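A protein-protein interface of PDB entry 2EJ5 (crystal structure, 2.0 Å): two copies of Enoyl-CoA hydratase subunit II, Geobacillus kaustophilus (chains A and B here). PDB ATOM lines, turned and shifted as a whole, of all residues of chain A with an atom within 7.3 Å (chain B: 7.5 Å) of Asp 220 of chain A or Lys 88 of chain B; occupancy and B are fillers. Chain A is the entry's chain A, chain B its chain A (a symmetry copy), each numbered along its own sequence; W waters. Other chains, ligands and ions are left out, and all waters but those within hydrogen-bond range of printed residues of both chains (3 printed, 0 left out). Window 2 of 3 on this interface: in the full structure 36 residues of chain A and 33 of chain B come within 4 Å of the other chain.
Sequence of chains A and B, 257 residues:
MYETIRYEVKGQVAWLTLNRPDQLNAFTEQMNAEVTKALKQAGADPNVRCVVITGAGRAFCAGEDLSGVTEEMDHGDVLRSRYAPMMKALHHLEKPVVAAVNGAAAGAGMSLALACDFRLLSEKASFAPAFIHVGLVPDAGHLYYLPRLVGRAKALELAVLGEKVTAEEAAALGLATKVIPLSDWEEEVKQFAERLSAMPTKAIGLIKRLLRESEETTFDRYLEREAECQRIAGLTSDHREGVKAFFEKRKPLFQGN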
ATOM      1  N   THR A 217      -8.944 -13.129   5.435  1.00  0.00           N
ATOM      2  CA  THR A 217      -9.255 -14.485   4.963  1.00  0.00           C
ATOM      3  C   THR A 217      -8.425 -14.905   3.720  1.00  0.00           C
ATOM      4  O   THR A 217      -7.718 -14.101   3.140  1.00  0.00           O
ATOM      5  CB  THR A 217     -10.826 -14.686   4.761  1.00  0.00           C
ATOM      6  OG1 THR A 217     -11.196 -16.054   5.028  1.00  0.00           O
ATOM      7  CG2 THR A 217     -11.277 -14.274   3.359  1.00  0.00           C
ATOM      8  N   THR A 218      -8.502 -16.166   3.332  1.00  0.00           N
ATOM      9  CA  THR A 218      -7.809 -16.652   2.140  1.00  0.00           C
ATOM     10  C   THR A 218      -8.629 -16.394   0.866  1.00  0.00           C
ATOM     11  O   THR A 218      -9.837 -16.178   0.937  1.00  0.00           O
ATOM     12  CB  THR A 218      -7.588 -18.160   2.204  1.00  0.00           C
ATOM     13  OG1 THR A 218      -8.865 -18.803   2.303  1.00  0.00           O
ATOM     14  CG2 THR A 218      -6.691 -18.566   3.403  1.00  0.00           C
ATOM     15  N   PHE A 219      -7.990 -16.454  -0.299  1.00  0.00           N
ATOM     16  CA  PHE A 219      -8.699 -16.220  -1.565  1.00  0.00           C
ATOM     17  C   PHE A 219      -9.985 -17.052  -1.733  1.00  0.00           C
ATOM     18  O   PHE A 219     -11.039 -16.515  -2.073  1.00  0.00           O
ATOM     19  CB  PHE A 219      -7.788 -16.502  -2.753  1.00  0.00           C
ATOM     20  CG  PHE A 219      -8.401 -16.150  -4.071  1.00  0.00           C
ATOM     21  CD1 PHE A 219      -8.658 -14.822  -4.391  1.00  0.00           C
ATOM     22  CD2 PHE A 219      -8.728 -17.133  -4.977  1.00  0.00           C
ATOM     23  CE1 PHE A 219      -9.225 -14.483  -5.586  1.00  0.00           C
ATOM     24  CE2 PHE A 219      -9.296 -16.816  -6.182  1.00  0.00           C
ATOM     25  CZ  PHE A 219      -9.552 -15.485  -6.495  1.00  0.00           C
ATOM     26  N   ASP A 220      -9.875 -18.370  -1.517  1.00  0.00           N
ATOM     27  CA  ASP A 220     -11.009 -19.268  -1.662  1.00  0.00           C
ATOM     28  C   ASP A 220     -12.182 -18.876  -0.764  1.00  0.00           C
ATOM     29  O   ASP A 220     -13.331 -18.821  -1.218  1.00  0.00           O
ATOM     30  CB  ASP A 220     -10.592 -20.710  -1.406  1.00  0.00           C
ATOM     31  CG  ASP A 220      -9.804 -21.301  -2.556  1.00  0.00           C
ATOM     32  OD1 ASP A 220      -9.955 -20.801  -3.698  1.00  0.00           O
ATOM     33  OD2 ASP A 220      -9.038 -22.278  -2.325  1.00  0.00           O
ATOM     34  N   ARG A 221     -11.901 -18.569   0.491  1.00  0.00           N
ATOM     35  CA  ARG A 221     -12.968 -18.221   1.403  1.00  0.00           C
ATOM     36  C   ARG A 221     -13.503 -16.845   1.047  1.00  0.00           C
ATOM     37  O   ARG A 221     -14.710 -16.629   1.099  1.00  0.00           O
ATOM     38  CB  ARG A 221     -12.489 -18.256   2.848  1.00  0.00           C
ATOM     39  CG  ARG A 221     -12.340 -19.689   3.376  1.00  0.00           C
ATOM     40  CD  ARG A 221     -11.614 -19.694   4.736  1.00  0.00           C
ATOM     41  NE  ARG A 221     -12.471 -19.225   5.827  1.00  0.00           N
ATOM     42  CZ  ARG A 221     -13.433 -19.947   6.415  1.00  0.00           C
ATOM     43  NH1 ARG A 221     -13.700 -21.193   6.039  1.00  0.00           N
ATOM     44  NH2 ARG A 221     -14.145 -19.410   7.394  1.00  0.00           N
ATOM     45  N   TYR A 222     -12.597 -15.946   0.654  1.00  0.00           N
ATOM     46  CA  TYR A 222     -12.995 -14.602   0.224  1.00  0.00           C
ATOM     47  C   TYR A 222     -14.123 -14.628  -0.835  1.00  0.00           C
ATOM     48  O   TYR A 222     -15.107 -13.901  -0.728  1.00  0.00           O
ATOM     49  CB  TYR A 222     -11.807 -13.793  -0.316  1.00  0.00           C
ATOM     50  CG  TYR A 222     -12.312 -12.452  -0.720  1.00  0.00           C
ATOM     51  CD1 TYR A 222     -12.524 -11.464   0.246  1.00  0.00           C
ATOM     52  CD2 TYR A 222     -12.673 -12.191  -2.055  1.00  0.00           C
ATOM     53  CE1 TYR A 222     -13.061 -10.220  -0.110  1.00  0.00           C
ATOM     54  CE2 TYR A 222     -13.222 -10.950  -2.411  1.00  0.00           C
ATOM     55  CZ  TYR A 222     -13.415  -9.993  -1.433  1.00  0.00           C
ATOM     56  OH  TYR A 222     -13.963  -8.797  -1.750  1.00  0.00           O
ATOM     57  N   LEU A 223     -13.955 -15.437  -1.867  1.00  0.00           N
ATOM     58  CA  LEU A 223     -14.981 -15.535  -2.918  1.00  0.00           C
ATOM     59  C   LEU A 223     -16.361 -15.981  -2.365  1.00  0.00           C
ATOM     60  O   LEU A 223     -17.387 -15.577  -2.892  1.00  0.00           O
ATOM     61  CB  LEU A 223     -14.565 -16.516  -4.030  1.00  0.00           C
ATOM     62  CG  LEU A 223     -13.258 -16.195  -4.783  1.00  0.00           C
ATOM     63  CD1 LEU A 223     -12.905 -17.172  -5.918  1.00  0.00           C
ATOM     64  CD2 LEU A 223     -13.410 -14.786  -5.341  1.00  0.00           C
ATOM     65  N   GLU A 224     -16.370 -16.849  -1.353  1.00  0.00           N
ATOM     66  CA  GLU A 224     -17.651 -17.257  -0.750  1.00  0.00           C
ATOM     67  C   GLU A 224     -18.282 -16.075   0.009  1.00  0.00           C
ATOM     68  O   GLU A 224     -19.484 -15.831  -0.128  1.00  0.00           O
ATOM     69  CB  GLU A 224     -17.516 -18.495   0.166  1.00  0.00           C
ATOM     70  CG  GLU A 224     -17.259 -19.831  -0.553  1.00  0.00           C
ATOM     71  CD  GLU A 224     -18.471 -20.392  -1.303  1.00  0.00           C
ATOM     72  OE1 GLU A 224     -19.586 -19.800  -1.243  1.00  0.00           O
ATOM     73  OE2 GLU A 224     -18.306 -21.444  -1.978  1.00  0.00           O
ATOM     74  N   ARG A 225     -17.461 -15.305   0.742  1.00  0.00           N
ATOM     75  CA  ARG A 225     -17.940 -14.078   1.411  1.00  0.00           C
ATOM     76  C   ARG A 225     -18.481 -13.058   0.382  1.00  0.00           C
ATOM     77  O   ARG A 225     -19.515 -12.407   0.585  1.00  0.00           O
ATOM     78  CB  ARG A 225     -16.817 -13.429   2.247  1.00  0.00           C
ATOM     79  CG  ARG A 225     -16.181 -14.338   3.357  1.00  0.00           C
ATOM     80  CD  ARG A 225     -17.177 -14.720   4.551  1.00  0.00           C
ATOM     81  NE  ARG A 225     -18.084 -15.818   4.197  1.00  0.00           N
ATOM     82  CZ  ARG A 225     -17.754 -17.115   4.141  1.00  0.00           C
ATOM     83  NH1 ARG A 225     -16.506 -17.526   4.387  1.00  0.00           N
ATOM     84  NH2 ARG A 225     -18.674 -18.015   3.805  1.00  0.00           N
ATOM     85  N   THR B  36     -12.679 -20.625 -18.324  1.00  0.00           N
ATOM     86  CA  THR B  36     -12.214 -21.589 -17.322  1.00  0.00           C
ATOM     87  C   THR B  36     -11.493 -22.744 -17.984  1.00  0.00           C
ATOM     88  O   THR B  36     -10.351 -23.059 -17.638  1.00  0.00           O
ATOM     89  CB  THR B  36     -13.393 -22.138 -16.415  1.00  0.00           C
ATOM     90  OG1 THR B  36     -14.027 -21.054 -15.728  1.00  0.00           O
ATOM     91  CG2 THR B  36     -12.910 -23.122 -15.364  1.00  0.00           C
ATOM     92  N   LEU B  39      -8.201 -21.656 -19.720  1.00  0.00           N
ATOM     93  CA  LEU B  39      -7.108 -21.420 -18.760  1.00  0.00           C
ATOM     94  C   LEU B  39      -6.529 -22.707 -18.289  1.00  0.00           C
ATOM     95  O   LEU B  39      -5.339 -22.820 -18.121  1.00  0.00           O
ATOM     96  CB  LEU B  39      -7.551 -20.593 -17.550  1.00  0.00           C
ATOM     97  CG  LEU B  39      -7.901 -19.129 -17.813  1.00  0.00           C
ATOM     98  CD1 LEU B  39      -8.465 -18.507 -16.538  1.00  0.00           C
ATOM     99  CD2 LEU B  39      -6.731 -18.286 -18.442  1.00  0.00           C
ATOM    100  N   LYS B  40      -7.380 -23.711 -18.073  1.00  0.00           N
ATOM    101  CA  LYS B  40      -6.895 -24.996 -17.583  1.00  0.00           C
ATOM    102  C   LYS B  40      -6.121 -25.694 -18.716  1.00  0.00           C
ATOM    103  O   LYS B  40      -5.118 -26.340 -18.463  1.00  0.00           O
ATOM    104  CB  LYS B  40      -8.068 -25.866 -17.050  1.00  0.00           C
ATOM    105  CG  LYS B  40      -8.818 -25.268 -15.825  1.00  0.00           C
ATOM    106  CD  LYS B  40     -10.084 -26.070 -15.475  1.00  0.00           C
ATOM    107  CE  LYS B  40     -10.708 -25.618 -14.127  1.00  0.00           C
ATOM    108  NZ  LYS B  40     -11.987 -26.375 -13.707  1.00  0.00           N
ATOM    109  N   ARG B  80     -20.998 -17.752  -7.493  1.00  0.00           N
ATOM    110  CA  ARG B  80     -20.398 -19.036  -7.114  1.00  0.00           C
ATOM    111  C   ARG B  80     -20.421 -20.053  -8.240  1.00  0.00           C
ATOM    112  O   ARG B  80     -19.517 -20.877  -8.348  1.00  0.00           O
ATOM    113  CB  ARG B  80     -20.940 -19.598  -5.779  1.00  0.00           C
ATOM    114  CG  ARG B  80     -22.274 -20.276  -5.816  1.00  0.00           C
ATOM    115  CD  ARG B  80     -22.627 -20.880  -4.413  1.00  0.00           C
ATOM    116  NE  ARG B  80     -22.381 -19.941  -3.313  1.00  0.00           N
ATOM    117  CZ  ARG B  80     -23.223 -18.982  -2.934  1.00  0.00           C
ATOM    118  NH1 ARG B  80     -24.379 -18.818  -3.561  1.00  0.00           N
ATOM    119  NH2 ARG B  80     -22.911 -18.183  -1.922  1.00  0.00           N
ATOM    120  N   TYR B  83     -18.561 -17.449 -11.918  1.00  0.00           N
ATOM    121  CA  TYR B  83     -17.320 -16.653 -11.788  1.00  0.00           C
ATOM    122  C   TYR B  83     -16.259 -17.321 -10.920  1.00  0.00           C
ATOM    123  O   TYR B  83     -15.091 -17.236 -11.228  1.00  0.00           O
ATOM    124  CB  TYR B  83     -17.628 -15.241 -11.262  1.00  0.00           C
ATOM    125  CG  TYR B  83     -18.221 -14.313 -12.275  1.00  0.00           C
ATOM    126  CD1 TYR B  83     -17.417 -13.413 -12.992  1.00  0.00           C
ATOM    127  CD2 TYR B  83     -19.600 -14.332 -12.547  1.00  0.00           C
ATOM    128  CE1 TYR B  83     -17.959 -12.548 -13.960  1.00  0.00           C
ATOM    129  CE2 TYR B  83     -20.158 -13.463 -13.518  1.00  0.00           C
ATOM    130  CZ  TYR B  83     -19.329 -12.583 -14.216  1.00  0.00           C
ATOM    131  OH  TYR B  83     -19.893 -11.715 -15.123  1.00  0.00           O
ATOM    132  N   ALA B  84     -16.664 -17.969  -9.825  1.00  0.00           N
ATOM    133  CA  ALA B  84     -15.717 -18.654  -8.926  1.00  0.00           C
ATOM    134  C   ALA B  84     -14.799 -19.678  -9.633  1.00  0.00           C
ATOM    135  O   ALA B  84     -13.580 -19.605  -9.469  1.00  0.00           O
ATOM    136  CB  ALA B  84     -16.443 -19.272  -7.689  1.00  0.00           C
ATOM    137  N   PRO B  85     -15.359 -20.600 -10.450  1.00  0.00           N
ATOM    138  CA  PRO B  85     -14.477 -21.528 -11.187  1.00  0.00           C
ATOM    139  C   PRO B  85     -13.448 -20.855 -12.122  1.00  0.00           C
ATOM    140  O   PRO B  85     -12.303 -21.350 -12.242  1.00  0.00           O
ATOM    141  CB  PRO B  85     -15.457 -22.366 -12.017  1.00  0.00           C
ATOM    142  CG  PRO B  85     -16.734 -22.304 -11.273  1.00  0.00           C
ATOM    143  CD  PRO B  85     -16.782 -20.894 -10.727  1.00  0.00           C
ATOM    144  N   MET B  86     -13.864 -19.773 -12.777  1.00  0.00           N
ATOM    145  CA  MET B  86     -13.033 -18.996 -13.697  1.00  0.00           C
ATOM    146  C   MET B  86     -11.908 -18.291 -12.921  1.00  0.00           C
ATOM    147  O   MET B  86     -10.739 -18.381 -13.290  1.00  0.00           O
ATOM    148  CB  MET B  86     -13.903 -17.973 -14.440  1.00  0.00           C
ATOM    149  CG  MET B  86     -13.198 -17.236 -15.651  1.00  0.00           C
ATOM    150  SD  MET B  86     -14.014 -15.878 -16.483  1.00  0.00           S
ATOM    151  CE  MET B  86     -14.201 -14.609 -15.209  1.00  0.00           C
ATOM    152  N   MET B  87     -12.270 -17.586 -11.854  1.00  0.00           N
ATOM    153  CA  MET B  87     -11.272 -16.880 -11.049  1.00  0.00           C
ATOM    154  C   MET B  87     -10.360 -17.833 -10.314  1.00  0.00           C
ATOM    155  O   MET B  87      -9.180 -17.533 -10.146  1.00  0.00           O
ATOM    156  CB  MET B  87     -11.931 -15.820 -10.118  1.00  0.00           C
ATOM    157  CG  MET B  87     -12.822 -14.761 -10.896  1.00  0.00           C
ATOM    158  SD  MET B  87     -12.085 -13.889 -12.310  1.00  0.00           S
ATOM    159  CE  MET B  87     -10.736 -13.047 -11.481  1.00  0.00           C
ATOM    160  N   LYS B  88     -10.857 -19.007  -9.911  1.00  0.00           N
ATOM    161  CA  LYS B  88      -9.978 -20.008  -9.282  1.00  0.00           C
ATOM    162  C   LYS B  88      -9.014 -20.599 -10.292  1.00  0.00           C
ATOM    163  O   LYS B  88      -7.844 -20.823  -9.969  1.00  0.00           O
ATOM    164  CB  LYS B  88     -10.759 -21.150  -8.619  1.00  0.00           C
ATOM    165  CG  LYS B  88     -11.634 -20.682  -7.477  1.00  0.00           C
ATOM    166  CD  LYS B  88     -12.276 -21.854  -6.795  1.00  0.00           C
ATOM    167  CE  LYS B  88     -12.801 -21.405  -5.472  1.00  0.00           C
ATOM    168  NZ  LYS B  88     -13.836 -22.372  -4.957  1.00  0.00           N
ATOM    169  N   ALA B  89      -9.504 -20.870 -11.515  1.00  0.00           N
ATOM    170  CA  ALA B  89      -8.600 -21.346 -12.575  1.00  0.00           C
ATOM    171  C   ALA B  89      -7.496 -20.307 -12.827  1.00  0.00           C
ATOM    172  O   ALA B  89      -6.330 -20.653 -12.922  1.00  0.00           O
ATOM    173  CB  ALA B  89      -9.362 -21.634 -13.893  1.00  0.00           C
ATOM    174  N   LEU B  90      -7.868 -19.043 -12.961  1.00  0.00           N
ATOM    175  CA  LEU B  90      -6.852 -17.997 -13.192  1.00  0.00           C
ATOM    176  C   LEU B  90      -5.896 -17.944 -12.027  1.00  0.00           C
ATOM    177  O   LEU B  90      -4.687 -17.878 -12.201  1.00  0.00           O
ATOM    178  CB  LEU B  90      -7.513 -16.645 -13.454  1.00  0.00           C
ATOM    179  CG  LEU B  90      -6.673 -15.407 -13.793  1.00  0.00           C
ATOM    180  CD1 LEU B  90      -5.681 -15.679 -14.964  1.00  0.00           C
ATOM    181  CD2 LEU B  90      -7.612 -14.214 -14.106  1.00  0.00           C
ATOM    182  N   HIS B  91      -6.437 -17.992 -10.822  1.00  0.00           N
ATOM    183  CA  HIS B  91      -5.644 -17.774  -9.611  1.00  0.00           C
ATOM    184  C   HIS B  91      -4.647 -18.913  -9.413  1.00  0.00           C
ATOM    185  O   HIS B  91      -3.549 -18.695  -8.920  1.00  0.00           O
ATOM    186  CB  HIS B  91      -6.609 -17.593  -8.413  1.00  0.00           C
ATOM    187  CG  HIS B  91      -5.935 -17.315  -7.110  1.00  0.00           C
ATOM    188  ND1 HIS B  91      -5.433 -18.311  -6.309  1.00  0.00           N
ATOM    189  CD2 HIS B  91      -5.640 -16.149  -6.484  1.00  0.00           C
ATOM    190  CE1 HIS B  91      -4.885 -17.779  -5.231  1.00  0.00           C
ATOM    191  NE2 HIS B  91      -4.993 -16.470  -5.312  1.00  0.00           N
ATOM    192  N   HIS B  92      -5.004 -20.125  -9.836  1.00  0.00           N
ATOM    193  CA  HIS B  92      -4.089 -21.255  -9.699  1.00  0.00           C
ATOM    194  C   HIS B  92      -3.203 -21.484 -10.927  1.00  0.00           C
ATOM    195  O   HIS B  92      -2.302 -22.262 -10.851  1.00  0.00           O
ATOM    196  CB  HIS B  92      -4.833 -22.551  -9.328  1.00  0.00           C
ATOM    197  CG  HIS B  92      -5.558 -22.478  -8.012  1.00  0.00           C
ATOM    198  ND1 HIS B  92      -6.647 -21.653  -7.801  1.00  0.00           N
ATOM    199  CD2 HIS B  92      -5.369 -23.150  -6.848  1.00  0.00           C
ATOM    200  CE1 HIS B  92      -7.085 -21.805  -6.564  1.00  0.00           C
ATOM    201  NE2 HIS B  92      -6.333 -22.715  -5.966  1.00  0.00           N
ATOM    202  N   LEU B  93      -3.459 -20.801 -12.040  1.00  0.00           N
ATOM    203  CA  LEU B  93      -2.621 -20.942 -13.234  1.00  0.00           C
ATOM    204  C   LEU B  93      -1.189 -20.435 -13.007  1.00  0.00           C
ATOM    205  O   LEU B  93      -0.991 -19.250 -12.679  1.00  0.00           O
ATOM    206  CB  LEU B  93      -3.279 -20.213 -14.423  1.00  0.00           C
ATOM    207  CG  LEU B  93      -2.592 -20.184 -15.798  1.00  0.00           C
ATOM    208  CD1 LEU B  93      -2.307 -21.621 -16.320  1.00  0.00           C
ATOM    209  CD2 LEU B  93      -3.459 -19.440 -16.748  1.00  0.00           C
ATOM    210  N   TYR B 144     -10.199  -8.409  -3.313  1.00  0.00           N
ATOM    211  CA  TYR B 144      -9.071  -9.186  -2.827  1.00  0.00           C
ATOM    212  C   TYR B 144      -7.831  -8.662  -3.541  1.00  0.00           C
ATOM    213  O   TYR B 144      -6.787  -8.428  -2.918  1.00  0.00           O
ATOM    214  CB  TYR B 144      -9.258 -10.691  -3.123  1.00  0.00           C
ATOM    215  CG  TYR B 144      -8.178 -11.539  -2.468  1.00  0.00           C
ATOM    216  CD1 TYR B 144      -8.298 -11.978  -1.129  1.00  0.00           C
ATOM    217  CD2 TYR B 144      -7.011 -11.882  -3.181  1.00  0.00           C
ATOM    218  CE1 TYR B 144      -7.293 -12.762  -0.527  1.00  0.00           C
ATOM    219  CE2 TYR B 144      -5.997 -12.650  -2.586  1.00  0.00           C
ATOM    220  CZ  TYR B 144      -6.140 -13.085  -1.271  1.00  0.00           C
ATOM    221  OH  TYR B 144      -5.106 -13.841  -0.697  1.00  0.00           O
ATOM    222  N   TYR B 145      -7.937  -8.466  -4.866  1.00  0.00           N
ATOM    223  CA  TYR B 145      -6.784  -7.991  -5.631  1.00  0.00           C
ATOM    224  C   TYR B 145      -6.430  -6.537  -5.434  1.00  0.00           C
ATOM    225  O   TYR B 145      -5.246  -6.169  -5.373  1.00  0.00           O
ATOM    226  CB  TYR B 145      -7.019  -8.234  -7.122  1.00  0.00           C
ATOM    227  CG  TYR B 145      -7.071  -9.727  -7.403  1.00  0.00           C
ATOM    228  CD1 TYR B 145      -5.945 -10.506  -7.239  1.00  0.00           C
ATOM    229  CD2 TYR B 145      -8.255 -10.349  -7.784  1.00  0.00           C
ATOM    230  CE1 TYR B 145      -5.990 -11.901  -7.466  1.00  0.00           C
ATOM    231  CE2 TYR B 145      -8.316 -11.742  -7.996  1.00  0.00           C
ATOM    232  CZ  TYR B 145      -7.177 -12.496  -7.854  1.00  0.00           C
ATOM    233  OH  TYR B 145      -7.202 -13.880  -8.075  1.00  0.00           O
ATOM    234  N   GLU B 216      -0.835 -15.671   2.104  1.00  0.00           N
ATOM    235  CA  GLU B 216      -1.671 -16.535   2.946  1.00  0.00           C
ATOM    236  C   GLU B 216      -1.004 -17.172   4.162  1.00  0.00           C
ATOM    237  O   GLU B 216      -1.711 -17.702   5.015  1.00  0.00           O
ATOM    238  CB  GLU B 216      -2.367 -17.627   2.103  1.00  0.00           C
ATOM    239  CG  GLU B 216      -3.176 -17.084   0.910  1.00  0.00           C
ATOM    240  CD  GLU B 216      -3.961 -18.172   0.175  1.00  0.00           C
ATOM    241  OE1 GLU B 216      -5.169 -17.955  -0.099  1.00  0.00           O
ATOM    242  OE2 GLU B 216      -3.375 -19.230  -0.144  1.00  0.00           O
HETATM  243  O   HOH W   1     -14.696 -20.445  -2.942  1.00  0.00           O
HETATM  244  O   HOH W   2      -6.839 -20.062  -1.174  1.00  0.00           O
HETATM  245  O   HOH W   3      -4.996 -14.371   2.034  1.00  0.00           O
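Among the printed residues, pairs that only touch across the chains: Thr 217 of chain A with Tyr 144 of chain B, Thr 218 of chain A with Glu 216 of chain B, Phe 219 of chain A with His 91 of chain B, Phe 219 of chain A with Tyr 144 of chain B, Phe 219 of chain A with Tyr 145 of chain B, Asp 220 of chain A with Lys 88 of chain B and Tyr 222 of chain A with Tyr 144 of chain B.
The backbone carbonyl oxygen (O) of Lys 88 of chain B sits at hydrogen-bond distance from a ring nitrogen (ND1) of His 92 of chain B (2.6 Å).
Of the 18 printed residues of chain B, 6 touch a printed residue of chain A. Hydrophobic or aromatic side chains of chain B within 4 Å of the printed part of chain A: His 91, Tyr 144 and Tyr 145. Printed residues of chain A that touch a printed residue of chain B: Thr 217, Thr 218, Phe 219, Asp 220, Tyr 222 and Glu 224. Hydrophobic or aromatic side chains of chain A that line the printed part of chain B: Phe 219 and Tyr 222. Among the printed residues, 9 pairs touch across the chains. Among the printed residues, Asp or Glu carboxylates within 4 Å of a Lys or Arg side-chain nitrogen of the other chain: Glu 224 of chain A with Arg 80 of chain B.
Water W1 lies within hydrogen-bond range of O of Asp 220 of chain A (2.7 Å) and NZ of Lys 88 of chain B (2.9 Å). Water W3 lies within hydrogen-bond range of the side-chain hydroxyl (OH) of Tyr 144 of chain B (2.8 Å) and the backbone carbonyl oxygen (O) of Thr 217 of chain A (3.0 Å). Water W2 lies within hydrogen-bond range of OE1 of Glu 216 of chain B (2.9 Å) and OD2 of Asp 220 of chain A (3.3 Å).
No position is printed for both chains.
N of Phe 219 of chain A lies within hydrogen-bond range of OE1 of Glu 216 of chain B (3.2 Å). The side-chain carboxylate (OE1) of Glu 224 of chain A lies within salt-bridge range of the guanidinium group (NE) of Arg 80 of chain B (3.5 Å).
Of the printed residues of chain B, Thr 218 of chain A touches Glu 216. Of the printed residues of chain B, Asp 220 of chain A touches Lys 88. Printed residues of chain B within 4 Å of Tyr 222 of chain A: Tyr 144. Thr 36 of chain B touches none of the printed residues of chain A. Met 87 of chain B touches none of the printed residues of chain A. Lys 88 of chain B touches just one residue of chain A: Asp 220.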
